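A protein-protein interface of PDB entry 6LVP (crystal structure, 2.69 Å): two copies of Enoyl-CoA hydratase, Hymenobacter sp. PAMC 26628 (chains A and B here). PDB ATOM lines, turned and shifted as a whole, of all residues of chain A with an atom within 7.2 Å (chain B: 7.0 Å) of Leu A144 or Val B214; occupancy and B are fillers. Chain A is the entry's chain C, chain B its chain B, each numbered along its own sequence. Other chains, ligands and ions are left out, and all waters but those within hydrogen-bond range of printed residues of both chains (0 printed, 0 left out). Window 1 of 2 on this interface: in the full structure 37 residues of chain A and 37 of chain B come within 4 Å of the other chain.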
ATOM      1  N   GLU A 118       1.271 -10.899  -9.348  1.00  0.00           N
ATOM      2  CA  GLU A 118       0.649 -10.087 -10.388  1.00  0.00           C
ATOM      3  C   GLU A 118       1.079  -8.627 -10.290  1.00  0.00           C
ATOM      4  O   GLU A 118       1.260  -7.956 -11.315  1.00  0.00           O
ATOM      5  CB  GLU A 118      -0.875 -10.203 -10.292  1.00  0.00           C
ATOM      6  CG  GLU A 118      -1.388 -11.629 -10.263  1.00  0.00           C
ATOM      7  CD  GLU A 118      -2.891 -11.731 -10.417  1.00  0.00           C
ATOM      8  OE1 GLU A 118      -3.607 -11.908  -9.395  1.00  0.00           O
ATOM      9  OE2 GLU A 118      -3.362 -11.647 -11.576  1.00  0.00           O
ATOM     10  N   PRO A 137      -0.994 -19.366  -6.804  1.00  0.00           N
ATOM     11  CA  PRO A 137      -1.659 -20.534  -6.204  1.00  0.00           C
ATOM     12  C   PRO A 137      -3.177 -20.452  -6.208  1.00  0.00           C
ATOM     13  O   PRO A 137      -3.833 -21.185  -5.457  1.00  0.00           O
ATOM     14  CB  PRO A 137      -1.118 -20.523  -4.770  1.00  0.00           C
ATOM     15  CG  PRO A 137      -0.980 -19.050  -4.469  1.00  0.00           C
ATOM     16  CD  PRO A 137      -0.565 -18.392  -5.781  1.00  0.00           C
ATOM     17  N   GLU A 138      -3.746 -19.578  -7.048  1.00  0.00           N
ATOM     18  CA  GLU A 138      -5.183 -19.313  -6.994  1.00  0.00           C
ATOM     19  C   GLU A 138      -6.020 -20.576  -7.217  1.00  0.00           C
ATOM     20  O   GLU A 138      -7.067 -20.739  -6.581  1.00  0.00           O
ATOM     21  CB  GLU A 138      -5.560 -18.238  -8.014  1.00  0.00           C
ATOM     22  CG  GLU A 138      -5.298 -16.800  -7.571  1.00  0.00           C
ATOM     23  CD  GLU A 138      -3.900 -16.294  -7.939  1.00  0.00           C
ATOM     24  OE1 GLU A 138      -2.989 -17.137  -8.142  1.00  0.00           O
ATOM     25  OE2 GLU A 138      -3.725 -15.046  -8.033  1.00  0.00           O
ATOM     26  N   VAL A 139      -5.595 -21.478  -8.111  1.00  0.00           N
ATOM     27  CA  VAL A 139      -6.435 -22.642  -8.417  1.00  0.00           C
ATOM     28  C   VAL A 139      -6.596 -23.544  -7.198  1.00  0.00           C
ATOM     29  O   VAL A 139      -7.587 -24.285  -7.107  1.00  0.00           O
ATOM     30  CB  VAL A 139      -5.900 -23.460  -9.627  1.00  0.00           C
ATOM     31  CG1 VAL A 139      -5.952 -22.642 -10.893  1.00  0.00           C
ATOM     32  CG2 VAL A 139      -4.487 -23.968  -9.382  1.00  0.00           C
ATOM     33  N   LEU A 141      -7.544 -22.632  -4.489  1.00  0.00           N
ATOM     34  CA  LEU A 141      -8.773 -22.161  -3.873  1.00  0.00           C
ATOM     35  C   LEU A 141      -9.970 -22.270  -4.799  1.00  0.00           C
ATOM     36  O   LEU A 141     -11.045 -21.787  -4.442  1.00  0.00           O
ATOM     37  CB  LEU A 141      -8.620 -20.708  -3.438  1.00  0.00           C
ATOM     38  CG  LEU A 141      -7.456 -20.400  -2.512  1.00  0.00           C
ATOM     39  CD1 LEU A 141      -7.317 -18.896  -2.391  1.00  0.00           C
ATOM     40  CD2 LEU A 141      -7.699 -21.039  -1.160  1.00  0.00           C
ATOM     41  N   GLY A 142      -9.816 -22.853  -5.989  1.00  0.00           N
ATOM     42  CA  GLY A 142     -10.890 -22.787  -6.962  1.00  0.00           C
ATOM     43  C   GLY A 142     -11.059 -21.409  -7.570  1.00  0.00           C
ATOM     44  O   GLY A 142     -12.168 -21.025  -7.961  1.00  0.00           O
ATOM     45  N   LEU A 143      -9.975 -20.649  -7.639  1.00  0.00           N
ATOM     46  CA  LEU A 143      -9.922 -19.330  -8.237  1.00  0.00           C
ATOM     47  C   LEU A 143      -8.909 -19.350  -9.365  1.00  0.00           C
ATOM     48  O   LEU A 143      -8.215 -20.344  -9.582  1.00  0.00           O
ATOM     49  CB  LEU A 143      -9.518 -18.285  -7.200  1.00  0.00           C
ATOM     50  CG  LEU A 143     -10.418 -17.087  -7.003  1.00  0.00           C
ATOM     51  CD1 LEU A 143     -11.860 -17.491  -7.198  1.00  0.00           C
ATOM     52  CD2 LEU A 143     -10.175 -16.577  -5.604  1.00  0.00           C
ATOM     53  N   LEU A 144      -8.818 -18.244 -10.080  1.00  0.00           N
ATOM     54  CA  LEU A 144      -7.768 -18.049 -11.066  1.00  0.00           C
ATOM     55  C   LEU A 144      -7.238 -16.636 -10.879  1.00  0.00           C
ATOM     56  O   LEU A 144      -7.893 -15.803 -10.241  1.00  0.00           O
ATOM     57  CB  LEU A 144      -8.273 -18.279 -12.502  1.00  0.00           C
ATOM     58  CG  LEU A 144      -8.977 -17.124 -13.216  1.00  0.00           C
ATOM     59  CD1 LEU A 144      -8.966 -17.306 -14.738  1.00  0.00           C
ATOM     60  CD2 LEU A 144     -10.401 -16.959 -12.706  1.00  0.00           C
ATOM     61  N   PRO A 145      -6.025 -16.350 -11.355  1.00  0.00           N
ATOM     62  CA  PRO A 145      -5.477 -14.996 -11.160  1.00  0.00           C
ATOM     63  C   PRO A 145      -6.389 -13.960 -11.804  1.00  0.00           C
ATOM     64  O   PRO A 145      -6.827 -14.120 -12.948  1.00  0.00           O
ATOM     65  CB  PRO A 145      -4.101 -15.064 -11.838  1.00  0.00           C
ATOM     66  CG  PRO A 145      -3.773 -16.547 -11.880  1.00  0.00           C
ATOM     67  CD  PRO A 145      -5.070 -17.250 -12.036  1.00  0.00           C
ATOM     68  N   GLY A 146      -6.703 -12.905 -11.050  1.00  0.00           N
ATOM     69  CA  GLY A 146      -7.714 -11.968 -11.500  1.00  0.00           C
ATOM     70  C   GLY A 146      -7.195 -10.566 -11.730  1.00  0.00           C
ATOM     71  O   GLY A 146      -7.968  -9.662 -12.077  1.00  0.00           O
ATOM     72  N   TYR A 147      -5.886 -10.367 -11.554  1.00  0.00           N
ATOM     73  CA  TYR A 147      -5.257  -9.054 -11.694  1.00  0.00           C
ATOM     74  C   TYR A 147      -4.293  -9.015 -12.871  1.00  0.00           C
ATOM     75  O   TYR A 147      -3.246  -8.369 -12.800  1.00  0.00           O
ATOM     76  CB  TYR A 147      -4.530  -8.650 -10.413  1.00  0.00           C
ATOM     77  CG  TYR A 147      -5.435  -8.442  -9.230  1.00  0.00           C
ATOM     78  CD1 TYR A 147      -6.717  -7.919  -9.395  1.00  0.00           C
ATOM     79  CD2 TYR A 147      -5.031  -8.793  -7.943  1.00  0.00           C
ATOM     80  CE1 TYR A 147      -7.555  -7.731  -8.319  1.00  0.00           C
ATOM     81  CE2 TYR A 147      -5.867  -8.613  -6.857  1.00  0.00           C
ATOM     82  CZ  TYR A 147      -7.120  -8.075  -7.055  1.00  0.00           C
ATOM     83  OH  TYR A 147      -7.953  -7.882  -5.992  1.00  0.00           O
ATOM     84  N   THR A 150      -3.116 -14.085 -15.986  1.00  0.00           N
ATOM     85  CA  THR A 150      -3.347 -14.877 -17.190  1.00  0.00           C
ATOM     86  C   THR A 150      -2.919 -14.172 -18.470  1.00  0.00           C
ATOM     87  O   THR A 150      -2.914 -14.812 -19.531  1.00  0.00           O
ATOM     88  CB  THR A 150      -4.827 -15.238 -17.322  1.00  0.00           C
ATOM     89  OG1 THR A 150      -5.581 -14.050 -17.617  1.00  0.00           O
ATOM     90  CG2 THR A 150      -5.330 -15.868 -16.036  1.00  0.00           C
ATOM     91  N   GLN A 151      -2.599 -12.878 -18.410  1.00  0.00           N
ATOM     92  CA  GLN A 151      -2.091 -12.133 -19.554  1.00  0.00           C
ATOM     93  C   GLN A 151      -0.595 -11.869 -19.445  1.00  0.00           C
ATOM     94  O   GLN A 151       0.142 -12.046 -20.420  1.00  0.00           O
ATOM     95  CB  GLN A 151      -2.848 -10.802 -19.685  1.00  0.00           C
ATOM     96  CG  GLN A 151      -4.377 -10.965 -19.713  1.00  0.00           C
ATOM     97  CD  GLN A 151      -4.820 -12.038 -20.701  1.00  0.00           C
ATOM     98  OE1 GLN A 151      -4.625 -11.902 -21.910  1.00  0.00           O
ATOM     99  NE2 GLN A 151      -5.397 -13.116 -20.191  1.00  0.00           N
ATOM    100  N   ALA A 162       3.777 -20.613 -18.358  1.00  0.00           N
ATOM    101  CA  ALA A 162       2.679 -19.906 -17.705  1.00  0.00           C
ATOM    102  C   ALA A 162       1.557 -20.872 -17.357  1.00  0.00           C
ATOM    103  O   ALA A 162       1.032 -20.857 -16.236  1.00  0.00           O
ATOM    104  CB  ALA A 162       2.161 -18.776 -18.590  1.00  0.00           C
ATOM    105  N   LEU A 163       1.183 -21.738 -18.305  1.00  0.00           N
ATOM    106  CA  LEU A 163       0.197 -22.768 -18.003  1.00  0.00           C
ATOM    107  C   LEU A 163       0.660 -23.655 -16.848  1.00  0.00           C
ATOM    108  O   LEU A 163      -0.078 -23.856 -15.875  1.00  0.00           O
ATOM    109  CB  LEU A 163      -0.109 -23.597 -19.253  1.00  0.00           C
ATOM    110  CG  LEU A 163      -1.035 -22.900 -20.270  1.00  0.00           C
ATOM    111  CD1 LEU A 163      -1.191 -23.680 -21.543  1.00  0.00           C
ATOM    112  CD2 LEU A 163      -2.392 -22.633 -19.662  1.00  0.00           C
ATOM    113  N   LEU A 165       2.763 -23.185 -14.367  1.00  0.00           N
ATOM    114  CA  LEU A 165       2.740 -22.517 -13.072  1.00  0.00           C
ATOM    115  C   LEU A 165       1.309 -22.246 -12.601  1.00  0.00           C
ATOM    116  O   LEU A 165       1.003 -22.377 -11.406  1.00  0.00           O
ATOM    117  CB  LEU A 165       3.547 -21.224 -13.141  1.00  0.00           C
ATOM    118  CG  LEU A 165       5.068 -21.342 -13.036  1.00  0.00           C
ATOM    119  CD1 LEU A 165       5.747 -20.125 -13.627  1.00  0.00           C
ATOM    120  CD2 LEU A 165       5.505 -21.521 -11.586  1.00  0.00           C
ATOM    121  N   MET A 166       0.414 -21.854 -13.514  1.00  0.00           N
ATOM    122  CA  MET A 166      -0.945 -21.535 -13.100  1.00  0.00           C
ATOM    123  C   MET A 166      -1.826 -22.771 -12.953  1.00  0.00           C
ATOM    124  O   MET A 166      -2.820 -22.719 -12.223  1.00  0.00           O
ATOM    125  CB  MET A 166      -1.573 -20.545 -14.083  1.00  0.00           C
ATOM    126  CG  MET A 166      -1.144 -19.095 -13.861  1.00  0.00           C
ATOM    127  SD  MET A 166      -1.822 -17.926 -15.082  1.00  0.00           S
ATOM    128  CE  MET A 166      -1.153 -18.556 -16.619  1.00  0.00           C
ATOM    129  N   LEU A 167      -1.485 -23.885 -13.602  1.00  0.00           N
ATOM    130  CA  LEU A 167      -2.260 -25.114 -13.429  1.00  0.00           C
ATOM    131  C   LEU A 167      -1.814 -25.942 -12.227  1.00  0.00           C
ATOM    132  O   LEU A 167      -2.646 -26.585 -11.585  1.00  0.00           O
ATOM    133  CB  LEU A 167      -2.186 -25.971 -14.695  1.00  0.00           C
ATOM    134  CG  LEU A 167      -2.865 -25.309 -15.896  1.00  0.00           C
ATOM    135  CD1 LEU A 167      -2.783 -26.179 -17.135  1.00  0.00           C
ATOM    136  CD2 LEU A 167      -4.308 -24.960 -15.563  1.00  0.00           C
ATOM    137  N   VAL B 209     -12.849 -26.488 -12.165  1.00  0.00           N
ATOM    138  CA  VAL B 209     -13.386 -25.391 -12.970  1.00  0.00           C
ATOM    139  C   VAL B 209     -12.345 -24.288 -13.117  1.00  0.00           C
ATOM    140  O   VAL B 209     -12.174 -23.710 -14.198  1.00  0.00           O
ATOM    141  CB  VAL B 209     -14.696 -24.860 -12.362  1.00  0.00           C
ATOM    142  CG1 VAL B 209     -15.214 -23.694 -13.169  1.00  0.00           C
ATOM    143  CG2 VAL B 209     -15.729 -25.956 -12.312  1.00  0.00           C
ATOM    144  N   ALA B 210     -11.617 -23.997 -12.042  1.00  0.00           N
ATOM    145  CA  ALA B 210     -10.537 -23.021 -12.110  1.00  0.00           C
ATOM    146  C   ALA B 210      -9.501 -23.398 -13.168  1.00  0.00           C
ATOM    147  O   ALA B 210      -9.062 -22.539 -13.939  1.00  0.00           O
ATOM    148  CB  ALA B 210      -9.890 -22.874 -10.733  1.00  0.00           C
ATOM    149  N   LEU B 211      -9.094 -24.673 -13.228  1.00  0.00           N
ATOM    150  CA  LEU B 211      -8.144 -25.084 -14.259  1.00  0.00           C
ATOM    151  C   LEU B 211      -8.636 -24.668 -15.635  1.00  0.00           C
ATOM    152  O   LEU B 211      -7.989 -23.873 -16.324  1.00  0.00           O
ATOM    153  CB  LEU B 211      -7.899 -26.590 -14.224  1.00  0.00           C
ATOM    154  CG  LEU B 211      -7.285 -27.169 -12.953  1.00  0.00           C
ATOM    155  CD1 LEU B 211      -6.976 -28.599 -13.230  1.00  0.00           C
ATOM    156  CD2 LEU B 211      -6.047 -26.430 -12.525  1.00  0.00           C
ATOM    157  N   GLY B 212      -9.812 -25.161 -16.028  1.00  0.00           N
ATOM    158  CA  GLY B 212     -10.383 -24.798 -17.314  1.00  0.00           C
ATOM    159  C   GLY B 212     -10.517 -23.299 -17.539  1.00  0.00           C
ATOM    160  O   GLY B 212     -10.401 -22.832 -18.674  1.00  0.00           O
ATOM    161  N   LEU B 213     -10.771 -22.524 -16.476  1.00  0.00           N
ATOM    162  CA  LEU B 213     -10.855 -21.073 -16.656  1.00  0.00           C
ATOM    163  C   LEU B 213      -9.481 -20.472 -16.934  1.00  0.00           C
ATOM    164  O   LEU B 213      -9.361 -19.540 -17.739  1.00  0.00           O
ATOM    165  CB  LEU B 213     -11.503 -20.404 -15.440  1.00  0.00           C
ATOM    166  CG  LEU B 213     -13.027 -20.566 -15.241  1.00  0.00           C
ATOM    167  CD1 LEU B 213     -13.480 -20.023 -13.870  1.00  0.00           C
ATOM    168  CD2 LEU B 213     -13.835 -19.950 -16.400  1.00  0.00           C
ATOM    169  N   VAL B 214      -8.431 -20.995 -16.290  1.00  0.00           N
ATOM    170  CA  VAL B 214      -7.081 -20.545 -16.612  1.00  0.00           C
ATOM    171  C   VAL B 214      -6.809 -20.747 -18.092  1.00  0.00           C
ATOM    172  O   VAL B 214      -6.386 -19.819 -18.794  1.00  0.00           O
ATOM    173  CB  VAL B 214      -6.031 -21.274 -15.750  1.00  0.00           C
ATOM    174  CG1 VAL B 214      -4.672 -21.175 -16.410  1.00  0.00           C
ATOM    175  CG2 VAL B 214      -5.965 -20.684 -14.345  1.00  0.00           C
ATOM    176  N   ILE B 215      -7.079 -21.957 -18.595  1.00  0.00           N
ATOM    177  CA  ILE B 215      -6.755 -22.285 -19.983  1.00  0.00           C
ATOM    178  C   ILE B 215      -7.489 -21.349 -20.941  1.00  0.00           C
ATOM    179  O   ILE B 215      -6.896 -20.817 -21.889  1.00  0.00           O
ATOM    180  CB  ILE B 215      -7.073 -23.764 -20.266  1.00  0.00           C
ATOM    181  CG1 ILE B 215      -6.075 -24.664 -19.540  1.00  0.00           C
ATOM    182  CG2 ILE B 215      -7.101 -24.060 -21.783  1.00  0.00           C
ATOM    183  CD1 ILE B 215      -6.581 -26.085 -19.322  1.00  0.00           C
ATOM    184  N   GLU B 216      -8.790 -21.132 -20.708  1.00  0.00           N
ATOM    185  CA  GLU B 216      -9.554 -20.192 -21.526  1.00  0.00           C
ATOM    186  C   GLU B 216      -8.925 -18.804 -21.501  1.00  0.00           C
ATOM    187  O   GLU B 216      -8.880 -18.119 -22.529  1.00  0.00           O
ATOM    188  CB  GLU B 216     -11.011 -20.110 -21.048  1.00  0.00           C
ATOM    189  CG  GLU B 216     -11.909 -21.285 -21.474  1.00  0.00           C
ATOM    190  CD  GLU B 216     -13.327 -21.273 -20.853  1.00  0.00           C
ATOM    191  OE1 GLU B 216     -13.943 -22.362 -20.768  1.00  0.00           O
ATOM    192  OE2 GLU B 216     -13.829 -20.189 -20.467  1.00  0.00           O
ATOM    193  N   CYS B 217      -8.409 -18.384 -20.345  1.00  0.00           N
ATOM    194  CA  CYS B 217      -7.898 -17.030 -20.228  1.00  0.00           C
ATOM    195  C   CYS B 217      -6.508 -16.848 -20.850  1.00  0.00           C
ATOM    196  O   CYS B 217      -6.263 -15.804 -21.473  1.00  0.00           O
ATOM    197  CB  CYS B 217      -7.932 -16.602 -18.766  1.00  0.00           C
ATOM    198  SG  CYS B 217      -9.623 -16.086 -18.279  1.00  0.00           S
ATOM    199  N   VAL B 218      -5.582 -17.817 -20.735  1.00  0.00           N
ATOM    200  CA  VAL B 218      -4.328 -17.589 -21.461  1.00  0.00           C
ATOM    201  C   VAL B 218      -4.570 -17.735 -22.964  1.00  0.00           C
ATOM    202  O   VAL B 218      -3.914 -17.064 -23.770  1.00  0.00           O
ATOM    203  CB  VAL B 218      -3.120 -18.457 -20.990  1.00  0.00           C
ATOM    204  CG1 VAL B 218      -3.273 -18.981 -19.563  1.00  0.00           C
ATOM    205  CG2 VAL B 218      -2.735 -19.548 -21.985  1.00  0.00           C
ATOM    206  N   ASN B 219      -5.551 -18.542 -23.367  1.00  0.00           N
ATOM    207  CA  ASN B 219      -5.877 -18.633 -24.788  1.00  0.00           C
ATOM    208  C   ASN B 219      -6.326 -17.284 -25.366  1.00  0.00           C
ATOM    209  O   ASN B 219      -5.947 -16.924 -26.487  1.00  0.00           O
ATOM    210  CB  ASN B 219      -6.943 -19.715 -25.007  1.00  0.00           C
ATOM    211  CG  ASN B 219      -6.352 -21.117 -25.028  1.00  0.00           C
ATOM    212  OD1 ASN B 219      -5.155 -21.283 -25.149  1.00  0.00           O
ATOM    213  ND2 ASN B 219      -7.191 -22.124 -24.906  1.00  0.00           N
ATOM    214  N   ALA B 220      -7.134 -16.519 -24.620  1.00  0.00           N
ATOM    215  CA  ALA B 220      -7.645 -15.259 -25.148  1.00  0.00           C
ATOM    216  C   ALA B 220      -6.552 -14.187 -25.263  1.00  0.00           C
ATOM    217  O   ALA B 220      -6.679 -13.244 -26.069  1.00  0.00           O
ATOM    218  CB  ALA B 220      -8.787 -14.764 -24.267  1.00  0.00           C
ATOM    219  N   ALA B 231     -11.795 -11.231 -20.433  1.00  0.00           N
ATOM    220  CA  ALA B 231     -12.005 -12.662 -20.220  1.00  0.00           C
ATOM    221  C   ALA B 231     -11.652 -13.056 -18.788  1.00  0.00           C
ATOM    222  O   ALA B 231     -12.393 -13.790 -18.121  1.00  0.00           O
ATOM    223  CB  ALA B 231     -11.159 -13.460 -21.217  1.00  0.00           C
ATOM    224  N   GLU B 232     -10.514 -12.560 -18.306  1.00  0.00           N
ATOM    225  CA  GLU B 232     -10.056 -12.862 -16.956  1.00  0.00           C
ATOM    226  C   GLU B 232     -11.028 -12.331 -15.904  1.00  0.00           C
ATOM    227  O   GLU B 232     -11.308 -13.019 -14.917  1.00  0.00           O
ATOM    228  CB  GLU B 232      -8.660 -12.269 -16.771  1.00  0.00           C
ATOM    229  CG  GLU B 232      -7.855 -12.816 -15.620  1.00  0.00           C
ATOM    230  CD  GLU B 232      -6.650 -11.930 -15.289  1.00  0.00           C
ATOM    231  OE1 GLU B 232      -6.858 -10.859 -14.656  1.00  0.00           O
ATOM    232  OE2 GLU B 232      -5.505 -12.292 -15.676  1.00  0.00           O
ATOM    233  N   THR B 233     -11.561 -11.116 -16.104  1.00  0.00           N
ATOM    234  CA  THR B 233     -12.533 -10.551 -15.170  1.00  0.00           C
ATOM    235  C   THR B 233     -13.831 -11.359 -15.170  1.00  0.00           C
ATOM    236  O   THR B 233     -14.383 -11.679 -14.104  1.00  0.00           O
ATOM    237  CB  THR B 233     -12.814  -9.076 -15.504  1.00  0.00           C
ATOM    238  OG1 THR B 233     -11.676  -8.274 -15.173  1.00  0.00           O
ATOM    239  CG2 THR B 233     -14.025  -8.539 -14.716  1.00  0.00           C
ATOM    240  N   GLU B 234     -14.335 -11.710 -16.360  1.00  0.00           N
ATOM    241  CA  GLU B 234     -15.549 -12.516 -16.416  1.00  0.00           C
ATOM    242  C   GLU B 234     -15.310 -13.917 -15.841  1.00  0.00           C
ATOM    243  O   GLU B 234     -16.185 -14.465 -15.160  1.00  0.00           O
ATOM    244  CB  GLU B 234     -16.087 -12.563 -17.855  1.00  0.00           C
ATOM    245  CG  GLU B 234     -17.631 -12.722 -17.961  1.00  0.00           C
ATOM    246  CD  GLU B 234     -18.445 -11.451 -17.566  1.00  0.00           C
ATOM    247  OE1 GLU B 234     -17.833 -10.407 -17.226  1.00  0.00           O
ATOM    248  OE2 GLU B 234     -19.705 -11.495 -17.596  1.00  0.00           O
ATOM    249  N   ALA B 235     -14.122 -14.502 -16.063  1.00  0.00           N
ATOM    250  CA  ALA B 235     -13.851 -15.828 -15.496  1.00  0.00           C
ATOM    251  C   ALA B 235     -13.670 -15.764 -13.980  1.00  0.00           C
ATOM    252  O   ALA B 235     -13.935 -16.744 -13.279  1.00  0.00           O
ATOM    253  CB  ALA B 235     -12.616 -16.461 -16.152  1.00  0.00           C
ATOM    254  N   PHE B 236     -13.234 -14.620 -13.468  1.00  0.00           N
ATOM    255  CA  PHE B 236     -12.995 -14.472 -12.043  1.00  0.00           C
ATOM    256  C   PHE B 236     -14.308 -14.373 -11.288  1.00  0.00           C
ATOM    257  O   PHE B 236     -14.444 -14.918 -10.185  1.00  0.00           O
ATOM    258  CB  PHE B 236     -12.135 -13.232 -11.816  1.00  0.00           C
ATOM    259  CG  PHE B 236     -11.597 -13.099 -10.425  1.00  0.00           C
ATOM    260  CD1 PHE B 236     -10.359 -13.647 -10.094  1.00  0.00           C
ATOM    261  CD2 PHE B 236     -12.308 -12.391  -9.458  1.00  0.00           C
ATOM    262  CE1 PHE B 236      -9.843 -13.499  -8.826  1.00  0.00           C
ATOM    263  CE2 PHE B 236     -11.816 -12.256  -8.184  1.00  0.00           C
ATOM    264  CZ  PHE B 236     -10.578 -12.809  -7.863  1.00  0.00           C
ATOM    265  N   GLY B 237     -15.281 -13.665 -11.869  1.00  0.00           N
ATOM    266  CA  GLY B 237     -16.631 -13.714 -11.347  1.00  0.00           C
ATOM    267  C   GLY B 237     -17.244 -15.097 -11.477  1.00  0.00           C
ATOM    268  O   GLY B 237     -17.972 -15.543 -10.585  1.00  0.00           O
ATOM    269  N   ARG B 238     -16.958 -15.790 -12.593  1.00  0.00           N
ATOM    270  CA  ARG B 238     -17.473 -17.143 -12.793  1.00  0.00           C
ATOM    271  C   ARG B 238     -16.985 -18.080 -11.693  1.00  0.00           C
ATOM    272  O   ARG B 238     -17.776 -18.837 -11.117  1.00  0.00           O
ATOM    273  CB  ARG B 238     -17.069 -17.682 -14.172  1.00  0.00           C
ATOM    274  CG  ARG B 238     -17.953 -17.244 -15.354  1.00  0.00           C
ATOM    275  CD  ARG B 238     -17.811 -18.185 -16.575  1.00  0.00           C
ATOM    276  NE  ARG B 238     -18.237 -19.549 -16.246  1.00  0.00           N
ATOM    277  CZ  ARG B 238     -17.785 -20.658 -16.830  1.00  0.00           C
ATOM    278  NH1 ARG B 238     -16.870 -20.586 -17.792  1.00  0.00           N
ATOM    279  NH2 ARG B 238     -18.239 -21.844 -16.438  1.00  0.00           N
ATOM    280  N   ALA B 239     -15.681 -18.040 -11.382  1.00  0.00           N
ATOM    281  CA  ALA B 239     -15.151 -18.920 -10.344  1.00  0.00           C
ATOM    282  C   ALA B 239     -15.849 -18.680  -9.022  1.00  0.00           C
ATOM    283  O   ALA B 239     -16.029 -19.619  -8.235  1.00  0.00           O
ATOM    284  CB  ALA B 239     -13.647 -18.718 -10.176  1.00  0.00           C
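O of Cys B217 is in hydrogen-bond range of NE2 of Gln A151 (3.1 Å).
N of Tyr A147 is in hydrogen-bond range of OE1 of Glu B232, 3.3 Å away.
The side-chain hydroxyl of Thr A150 lies within hydrogen-bond range of the side-chain carboxylate of Glu B232 (2.6 Å).
The backbone carbonyl oxygen (O) of Gly A146 lies close to the side-chain carboxylate (OE1) of Glu B232 (3.1 Å).
The side-chain sulfur (SG) of Cys B217 lies close to the backbone carbonyl oxygen (O) of Leu B213 (3.5 Å).
SG of Cys B217 is in hydrogen-bond range of O of Ala B231, at 3.6 Å.
SG of Cys B217 lies close to N of Glu B232 (3.6 Å).
OE2 of Glu A118 lies within hydrogen-bond range of N of Tyr A147 (2.8 Å).
The backbone carbonyl oxygen (O) of Glu A138 is in hydrogen-bond range of the backbone NH (N) of Leu A143 (3.1 Å).
The side-chain hydroxyl (OG1) of Thr A150 lies within hydrogen-bond range of the side-chain amide nitrogen (NE2) of Gln A151 (2.7 Å).
Among the printed residues, merely in contact across the chains: Val A139 with Ala B210 (3.9 Å), Val A139 with Val B214 (3.97 Å), Gly A142 with Ala B210 (3.7 Å), Gly A142 with Ala B239 (3.5 Å), Leu A143 with Ala B210 (3.2 Å), Leu A143 with Ala B239 (3.7 Å), Leu A144 with Leu B213 (3.8 Å), Leu A144 with Val B214 (3.8 Å), Leu A144 with Cys B217 (3.8 Å), Leu A144 with Ala B235 (3.6 Å), Leu A144 with Phe B236 (3.3 Å), Pro A145 with Glu B232 (3.1 Å), Gly A146 with Phe B236 (3.4 Å), Thr A150 with Cys B217 (3.7 Å), Thr A150 with Val B218 (3.7 Å), Leu A163 with Val B218 (3.8 Å), Met A166 with Val B214 (3.9 Å), Met A166 with Val B218 (3.7 Å), Leu A167 with Leu B211 (3.5 Å) and Leu A167 with Val B214 (3.9 Å).
Leu A144 touches five residues of chain B.
Of the printed residues of chain B, Met A166 touches Val B214 and Val B218.
Of the printed residues of chain B, Leu A167 touches Leu B211 (3.5 Å) and Val B214 (3.9 Å).
Of the printed residues of chain A, Leu B211 touches Leu A167.
The nearest residue of chain B that does not touch Leu A144 is Ala B239 (4.5 Å).
Of the 18 printed residues of chain A, 12 touch a printed residue of chain B.
Printed residues of chain B that touch a printed residue of chain A: Ala B210, Leu B211, Leu B213, Val B214, Cys B217, Val B218, Glu B232, Ala B235, Phe B236 and Ala B239.
Hydrophobic or aromatic side chains of chain B within 4 Å of the printed part of chain A: Ala B210, Leu B211, Val B214, Val B218, Phe B236 and Ala B239.
Among the printed residues, 24 pairs touch across the chains.
Among the printed residues, no Asp or Glu carboxylate lies within 4 Å of a Lys or Arg side-chain nitrogen of the other chain.
No position is printed for both chains.
Of the 24 pairs that touch across the chains among the printed residues, none has its exchanged pair printed and touching as well.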
